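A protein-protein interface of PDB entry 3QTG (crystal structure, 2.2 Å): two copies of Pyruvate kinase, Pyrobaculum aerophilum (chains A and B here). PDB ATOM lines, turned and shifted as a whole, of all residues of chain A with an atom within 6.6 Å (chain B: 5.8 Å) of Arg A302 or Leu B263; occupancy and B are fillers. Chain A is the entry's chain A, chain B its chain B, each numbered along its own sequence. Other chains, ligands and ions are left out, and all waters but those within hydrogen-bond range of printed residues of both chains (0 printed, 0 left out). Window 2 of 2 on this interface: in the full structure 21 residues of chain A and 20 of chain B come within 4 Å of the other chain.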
ATOM      1  N   ILE A 299      30.864 -29.362  -0.110  1.00  0.00           N
ATOM      2  CA  ILE A 299      29.910 -28.256   0.042  1.00  0.00           C
ATOM      3  C   ILE A 299      28.861 -28.649   1.096  1.00  0.00           C
ATOM      4  O   ILE A 299      28.400 -29.791   1.108  1.00  0.00           O
ATOM      5  CB  ILE A 299      29.181 -27.917  -1.286  1.00  0.00           C
ATOM      6  CG1 ILE A 299      30.139 -27.896  -2.494  1.00  0.00           C
ATOM      7  CG2 ILE A 299      28.400 -26.607  -1.170  1.00  0.00           C
ATOM      8  CD1 ILE A 299      31.212 -26.817  -2.458  1.00  0.00           C
ATOM      9  N   PRO A 300      28.483 -27.712   1.989  1.00  0.00           N
ATOM     10  CA  PRO A 300      27.423 -28.092   2.917  1.00  0.00           C
ATOM     11  C   PRO A 300      26.031 -27.944   2.275  1.00  0.00           C
ATOM     12  O   PRO A 300      25.888 -27.342   1.197  1.00  0.00           O
ATOM     13  CB  PRO A 300      27.613 -27.088   4.064  1.00  0.00           C
ATOM     14  CG  PRO A 300      28.088 -25.857   3.372  1.00  0.00           C
ATOM     15  CD  PRO A 300      28.954 -26.334   2.234  1.00  0.00           C
ATOM     16  N   THR A 301      25.023 -28.513   2.927  1.00  0.00           N
ATOM     17  CA  THR A 301      23.634 -28.305   2.530  1.00  0.00           C
ATOM     18  C   THR A 301      23.203 -26.881   2.923  1.00  0.00           C
ATOM     19  O   THR A 301      23.798 -26.267   3.813  1.00  0.00           O
ATOM     20  CB  THR A 301      22.700 -29.310   3.205  1.00  0.00           C
ATOM     21  OG1 THR A 301      22.460 -28.897   4.557  1.00  0.00           O
ATOM     22  CG2 THR A 301      23.287 -30.776   3.177  1.00  0.00           C
ATOM     23  N   ARG A 302      22.181 -26.370   2.237  1.00  0.00           N
ATOM     24  CA  ARG A 302      21.545 -25.086   2.564  1.00  0.00           C
ATOM     25  C   ARG A 302      21.068 -24.958   4.020  1.00  0.00           C
ATOM     26  O   ARG A 302      21.214 -23.901   4.635  1.00  0.00           O
ATOM     27  CB  ARG A 302      20.394 -24.826   1.606  1.00  0.00           C
ATOM     28  CG  ARG A 302      20.903 -24.417   0.214  1.00  0.00           C
ATOM     29  CD  ARG A 302      19.796 -24.297  -0.809  1.00  0.00           C
ATOM     30  NE  ARG A 302      20.341 -24.106  -2.157  1.00  0.00           N
ATOM     31  CZ  ARG A 302      20.655 -25.100  -2.995  1.00  0.00           C
ATOM     32  NH1 ARG A 302      20.464 -26.364  -2.639  1.00  0.00           N
ATOM     33  NH2 ARG A 302      21.154 -24.828  -4.196  1.00  0.00           N
ATOM     34  N   ALA A 303      20.507 -26.031   4.559  1.00  0.00           N
ATOM     35  CA  ALA A 303      20.031 -26.033   5.939  1.00  0.00           C
ATOM     36  C   ALA A 303      21.187 -25.848   6.923  1.00  0.00           C
ATOM     37  O   ALA A 303      21.027 -25.159   7.924  1.00  0.00           O
ATOM     38  CB  ALA A 303      19.248 -27.311   6.243  1.00  0.00           C
ATOM     39  N   GLU A 304      22.337 -26.457   6.625  1.00  0.00           N
ATOM     40  CA  GLU A 304      23.540 -26.315   7.458  1.00  0.00           C
ATOM     41  C   GLU A 304      24.099 -24.905   7.429  1.00  0.00           C
ATOM     42  O   GLU A 304      24.548 -24.402   8.452  1.00  0.00           O
ATOM     43  CB  GLU A 304      24.624 -27.308   7.042  1.00  0.00           C
ATOM     44  CG  GLU A 304      24.197 -28.758   7.254  1.00  0.00           C
ATOM     45  CD  GLU A 304      25.255 -29.763   6.818  1.00  0.00           C
ATOM     46  OE1 GLU A 304      26.010 -29.475   5.871  1.00  0.00           O
ATOM     47  OE2 GLU A 304      25.320 -30.840   7.445  1.00  0.00           O
ATOM     48  N   ILE A 305      24.058 -24.266   6.261  1.00  0.00           N
ATOM     49  CA  ILE A 305      24.405 -22.845   6.150  1.00  0.00           C
ATOM     50  C   ILE A 305      23.460 -21.979   7.006  1.00  0.00           C
ATOM     51  O   ILE A 305      23.923 -21.176   7.793  1.00  0.00           O
ATOM     52  CB  ILE A 305      24.426 -22.367   4.664  1.00  0.00           C
ATOM     53  CG1 ILE A 305      25.604 -23.020   3.917  1.00  0.00           C
ATOM     54  CG2 ILE A 305      24.473 -20.841   4.576  1.00  0.00           C
ATOM     55  CD1 ILE A 305      25.404 -23.174   2.433  1.00  0.00           C
ATOM     56  N   ASN A 306      22.149 -22.143   6.862  1.00  0.00           N
ATOM     57  CA  ASN A 306      21.222 -21.415   7.739  1.00  0.00           C
ATOM     58  C   ASN A 306      21.464 -21.673   9.251  1.00  0.00           C
ATOM     59  O   ASN A 306      21.448 -20.729  10.046  1.00  0.00           O
ATOM     60  CB  ASN A 306      19.769 -21.684   7.361  1.00  0.00           C
ATOM     61  CG  ASN A 306      19.386 -21.060   6.029  1.00  0.00           C
ATOM     62  OD1 ASN A 306      18.904 -21.745   5.115  1.00  0.00           O
ATOM     63  ND2 ASN A 306      19.579 -19.759   5.910  1.00  0.00           N
ATOM     64  N   ASP A 307      21.702 -22.937   9.616  1.00  0.00           N
ATOM     65  CA  ASP A 307      22.016 -23.350  11.010  1.00  0.00           C
ATOM     66  C   ASP A 307      23.229 -22.602  11.596  1.00  0.00           C
ATOM     67  O   ASP A 307      23.128 -21.975  12.651  1.00  0.00           O
ATOM     68  CB  ASP A 307      22.229 -24.866  11.053  1.00  0.00           C
ATOM     69  CG  ASP A 307      22.259 -25.443  12.474  1.00  0.00           C
ATOM     70  OD1 ASP A 307      21.938 -24.730  13.453  1.00  0.00           O
ATOM     71  OD2 ASP A 307      22.611 -26.645  12.599  1.00  0.00           O
ATOM     72  N   TRP A 337      34.364 -23.159   4.509  1.00  0.00           N
ATOM     73  CA  TRP A 337      32.932 -22.844   4.540  1.00  0.00           C
ATOM     74  C   TRP A 337      32.442 -22.236   5.861  1.00  0.00           C
ATOM     75  O   TRP A 337      31.600 -21.338   5.846  1.00  0.00           O
ATOM     76  CB  TRP A 337      32.103 -24.066   4.171  1.00  0.00           C
ATOM     77  CG  TRP A 337      31.842 -24.132   2.710  1.00  0.00           C
ATOM     78  CD1 TRP A 337      32.491 -24.915   1.787  1.00  0.00           C
ATOM     79  CD2 TRP A 337      30.877 -23.371   1.981  1.00  0.00           C
ATOM     80  NE1 TRP A 337      31.978 -24.692   0.541  1.00  0.00           N
ATOM     81  CE2 TRP A 337      30.989 -23.750   0.623  1.00  0.00           C
ATOM     82  CE3 TRP A 337      29.918 -22.414   2.344  1.00  0.00           C
ATOM     83  CZ2 TRP A 337      30.176 -23.203  -0.380  1.00  0.00           C
ATOM     84  CZ3 TRP A 337      29.113 -21.861   1.343  1.00  0.00           C
ATOM     85  CH2 TRP A 337      29.249 -22.261  -0.003  1.00  0.00           C
ATOM     86  N   GLY B 258      17.855 -18.591  -4.616  1.00  0.00           N
ATOM     87  CA  GLY B 258      19.178 -19.171  -4.381  1.00  0.00           C
ATOM     88  C   GLY B 258      20.045 -19.205  -5.630  1.00  0.00           C
ATOM     89  O   GLY B 258      21.273 -19.214  -5.548  1.00  0.00           O
ATOM     90  N   TYR B 261      21.941 -15.728  -5.909  1.00  0.00           N
ATOM     91  CA  TYR B 261      22.819 -15.406  -4.788  1.00  0.00           C
ATOM     92  C   TYR B 261      23.732 -16.574  -4.455  1.00  0.00           C
ATOM     93  O   TYR B 261      23.457 -17.712  -4.833  1.00  0.00           O
ATOM     94  CB  TYR B 261      21.982 -15.007  -3.563  1.00  0.00           C
ATOM     95  CG  TYR B 261      21.299 -13.689  -3.746  1.00  0.00           C
ATOM     96  CD1 TYR B 261      21.957 -12.499  -3.456  1.00  0.00           C
ATOM     97  CD2 TYR B 261      19.998 -13.621  -4.235  1.00  0.00           C
ATOM     98  CE1 TYR B 261      21.337 -11.282  -3.638  1.00  0.00           C
ATOM     99  CE2 TYR B 261      19.371 -12.401  -4.425  1.00  0.00           C
ATOM    100  CZ  TYR B 261      20.048 -11.237  -4.123  1.00  0.00           C
ATOM    101  OH  TYR B 261      19.428 -10.028  -4.317  1.00  0.00           O
ATOM    102  N   GLY B 262      24.822 -16.300  -3.755  1.00  0.00           N
ATOM    103  CA  GLY B 262      25.649 -17.386  -3.224  1.00  0.00           C
ATOM    104  C   GLY B 262      24.855 -18.113  -2.146  1.00  0.00           C
ATOM    105  O   GLY B 262      23.905 -17.561  -1.572  1.00  0.00           O
ATOM    106  N   LEU B 263      25.234 -19.356  -1.875  1.00  0.00           N
ATOM    107  CA  LEU B 263      24.572 -20.155  -0.843  1.00  0.00           C
ATOM    108  C   LEU B 263      24.681 -19.472   0.539  1.00  0.00           C
ATOM    109  O   LEU B 263      23.709 -19.413   1.296  1.00  0.00           O
ATOM    110  CB  LEU B 263      25.162 -21.573  -0.835  1.00  0.00           C
ATOM    111  CG  LEU B 263      24.922 -22.508  -2.039  1.00  0.00           C
ATOM    112  CD1 LEU B 263      26.120 -23.445  -2.255  1.00  0.00           C
ATOM    113  CD2 LEU B 263      23.647 -23.313  -1.865  1.00  0.00           C
ATOM    114  N   ASP B 264      25.858 -18.907   0.819  1.00  0.00           N
ATOM    115  CA  ASP B 264      26.151 -18.188   2.071  1.00  0.00           C
ATOM    116  C   ASP B 264      25.537 -16.780   2.182  1.00  0.00           C
ATOM    117  O   ASP B 264      25.533 -16.183   3.268  1.00  0.00           O
ATOM    118  CB  ASP B 264      27.676 -18.120   2.292  1.00  0.00           C
ATOM    119  CG  ASP B 264      28.408 -17.325   1.188  1.00  0.00           C
ATOM    120  OD1 ASP B 264      28.111 -17.509  -0.009  1.00  0.00           O
ATOM    121  OD2 ASP B 264      29.290 -16.508   1.517  1.00  0.00           O
ATOM    122  N   ALA B 265      25.030 -16.254   1.065  1.00  0.00           N
ATOM    123  CA  ALA B 265      24.454 -14.908   1.017  1.00  0.00           C
ATOM    124  C   ALA B 265      22.935 -14.870   1.229  1.00  0.00           C
ATOM    125  O   ALA B 265      22.367 -13.812   1.511  1.00  0.00           O
ATOM    126  CB  ALA B 265      24.814 -14.227  -0.319  1.00  0.00           C
ATOM    127  N   LEU B 266      22.289 -16.019   1.077  1.00  0.00           N
ATOM    128  CA  LEU B 266      20.831 -16.098   1.082  1.00  0.00           C
ATOM    129  C   LEU B 266      20.147 -15.846   2.450  1.00  0.00           C
ATOM    130  O   LEU B 266      19.044 -15.310   2.475  1.00  0.00           O
ATOM    131  CB  LEU B 266      20.376 -17.435   0.463  1.00  0.00           C
ATOM    132  CG  LEU B 266      18.899 -17.621   0.084  1.00  0.00           C
ATOM    133  CD1 LEU B 266      18.435 -16.607  -0.954  1.00  0.00           C
ATOM    134  CD2 LEU B 266      18.611 -19.050  -0.386  1.00  0.00           C
ATOM    135  N   PRO B 267      20.757 -16.289   3.580  1.00  0.00           N
ATOM    136  CA  PRO B 267      20.188 -15.952   4.894  1.00  0.00           C
ATOM    137  C   PRO B 267      19.990 -14.459   5.193  1.00  0.00           C
ATOM    138  O   PRO B 267      18.995 -14.098   5.816  1.00  0.00           O
ATOM    139  CB  PRO B 267      21.195 -16.569   5.877  1.00  0.00           C
ATOM    140  CG  PRO B 267      21.807 -17.718   5.102  1.00  0.00           C
ATOM    141  CD  PRO B 267      21.922 -17.198   3.709  1.00  0.00           C
ATOM    142  N   GLN B 289      12.535 -25.638   0.055  1.00  0.00           N
ATOM    143  CA  GLN B 289      13.780 -25.997   0.739  1.00  0.00           C
ATOM    144  C   GLN B 289      13.665 -25.867   2.262  1.00  0.00           C
ATOM    145  O   GLN B 289      14.556 -25.301   2.925  1.00  0.00           O
ATOM    146  CB  GLN B 289      14.938 -25.120   0.232  1.00  0.00           C
ATOM    147  CG  GLN B 289      15.246 -25.256  -1.271  1.00  0.00           C
ATOM    148  CD  GLN B 289      16.425 -24.372  -1.724  1.00  0.00           C
ATOM    149  OE1 GLN B 289      16.821 -23.411  -1.038  1.00  0.00           O
ATOM    150  NE2 GLN B 289      16.997 -24.708  -2.886  1.00  0.00           N
ATOM    151  N   ASP B 292      13.588 -30.455   2.756  1.00  0.00           N
ATOM    152  CA  ASP B 292      14.039 -31.105   1.517  1.00  0.00           C
ATOM    153  C   ASP B 292      14.441 -32.587   1.598  1.00  0.00           C
ATOM    154  O   ASP B 292      14.045 -33.362   0.735  1.00  0.00           O
ATOM    155  CB  ASP B 292      15.194 -30.309   0.895  1.00  0.00           C
ATOM    156  CG  ASP B 292      14.782 -29.568  -0.374  1.00  0.00           C
ATOM    157  OD1 ASP B 292      13.594 -29.666  -0.793  1.00  0.00           O
ATOM    158  OD2 ASP B 292      15.665 -28.889  -0.961  1.00  0.00           O
ATOM    159  N   ASP B 307      16.702 -24.844  10.965  1.00  0.00           N
ATOM    160  CA  ASP B 307      16.290 -23.907   9.901  1.00  0.00           C
ATOM    161  C   ASP B 307      14.795 -23.601   9.985  1.00  0.00           C
ATOM    162  O   ASP B 307      14.397 -22.434   9.955  1.00  0.00           O
ATOM    163  CB  ASP B 307      16.666 -24.519   8.545  1.00  0.00           C
ATOM    164  CG  ASP B 307      16.446 -23.584   7.361  1.00  0.00           C
ATOM    165  OD1 ASP B 307      16.246 -22.348   7.536  1.00  0.00           O
ATOM    166  OD2 ASP B 307      16.477 -24.127   6.223  1.00  0.00           O
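The guanidinium group (NE) of Arg A302 sits close to the side-chain amide nitrogen (NE2) of Gln B289 (3.5 Å).
The backbone carbonyl oxygen (O) of Arg A302 lies close to the side-chain amide oxygen (OD1) of Asn A306 (3.2 Å).
Leu B263 touches Arg A302 (CD2 to NE, 3.4 Å).
Leu B263 touches Ile A305.
CG of Pro B267 touches ND2 of Asn A306 (3.1 Å).
OD1 of Asn A306 touches OD2 of Asp B307 (3.6 Å).
Printed residues of chain B within 4 Å of Arg A302: Leu B263 (3.4 Å) and Gln B289 (3.1 Å).
Leu B263 touches just these residues of chain A: Arg A302 and Ile A305.
Printed residues of chain A within 4 Å of Gln B289: Arg A302.
Of the printed residues of chain B, Ile A305 touches Leu B263.
Ala B265 touches none of the printed residues of chain A.
Hydrophobic or aromatic side chains of chain A within 4 Å of the printed part of chain B: Ile A305.
Of the 11 printed residues of chain B, 4 touch a printed residue of chain A.
Among the printed residues, 5 pairs touch across the chains.
Position printed for both chains: 307.
Of the 5 pairs that touch across the chains among the printed residues, none has its exchanged pair printed and touching as well.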
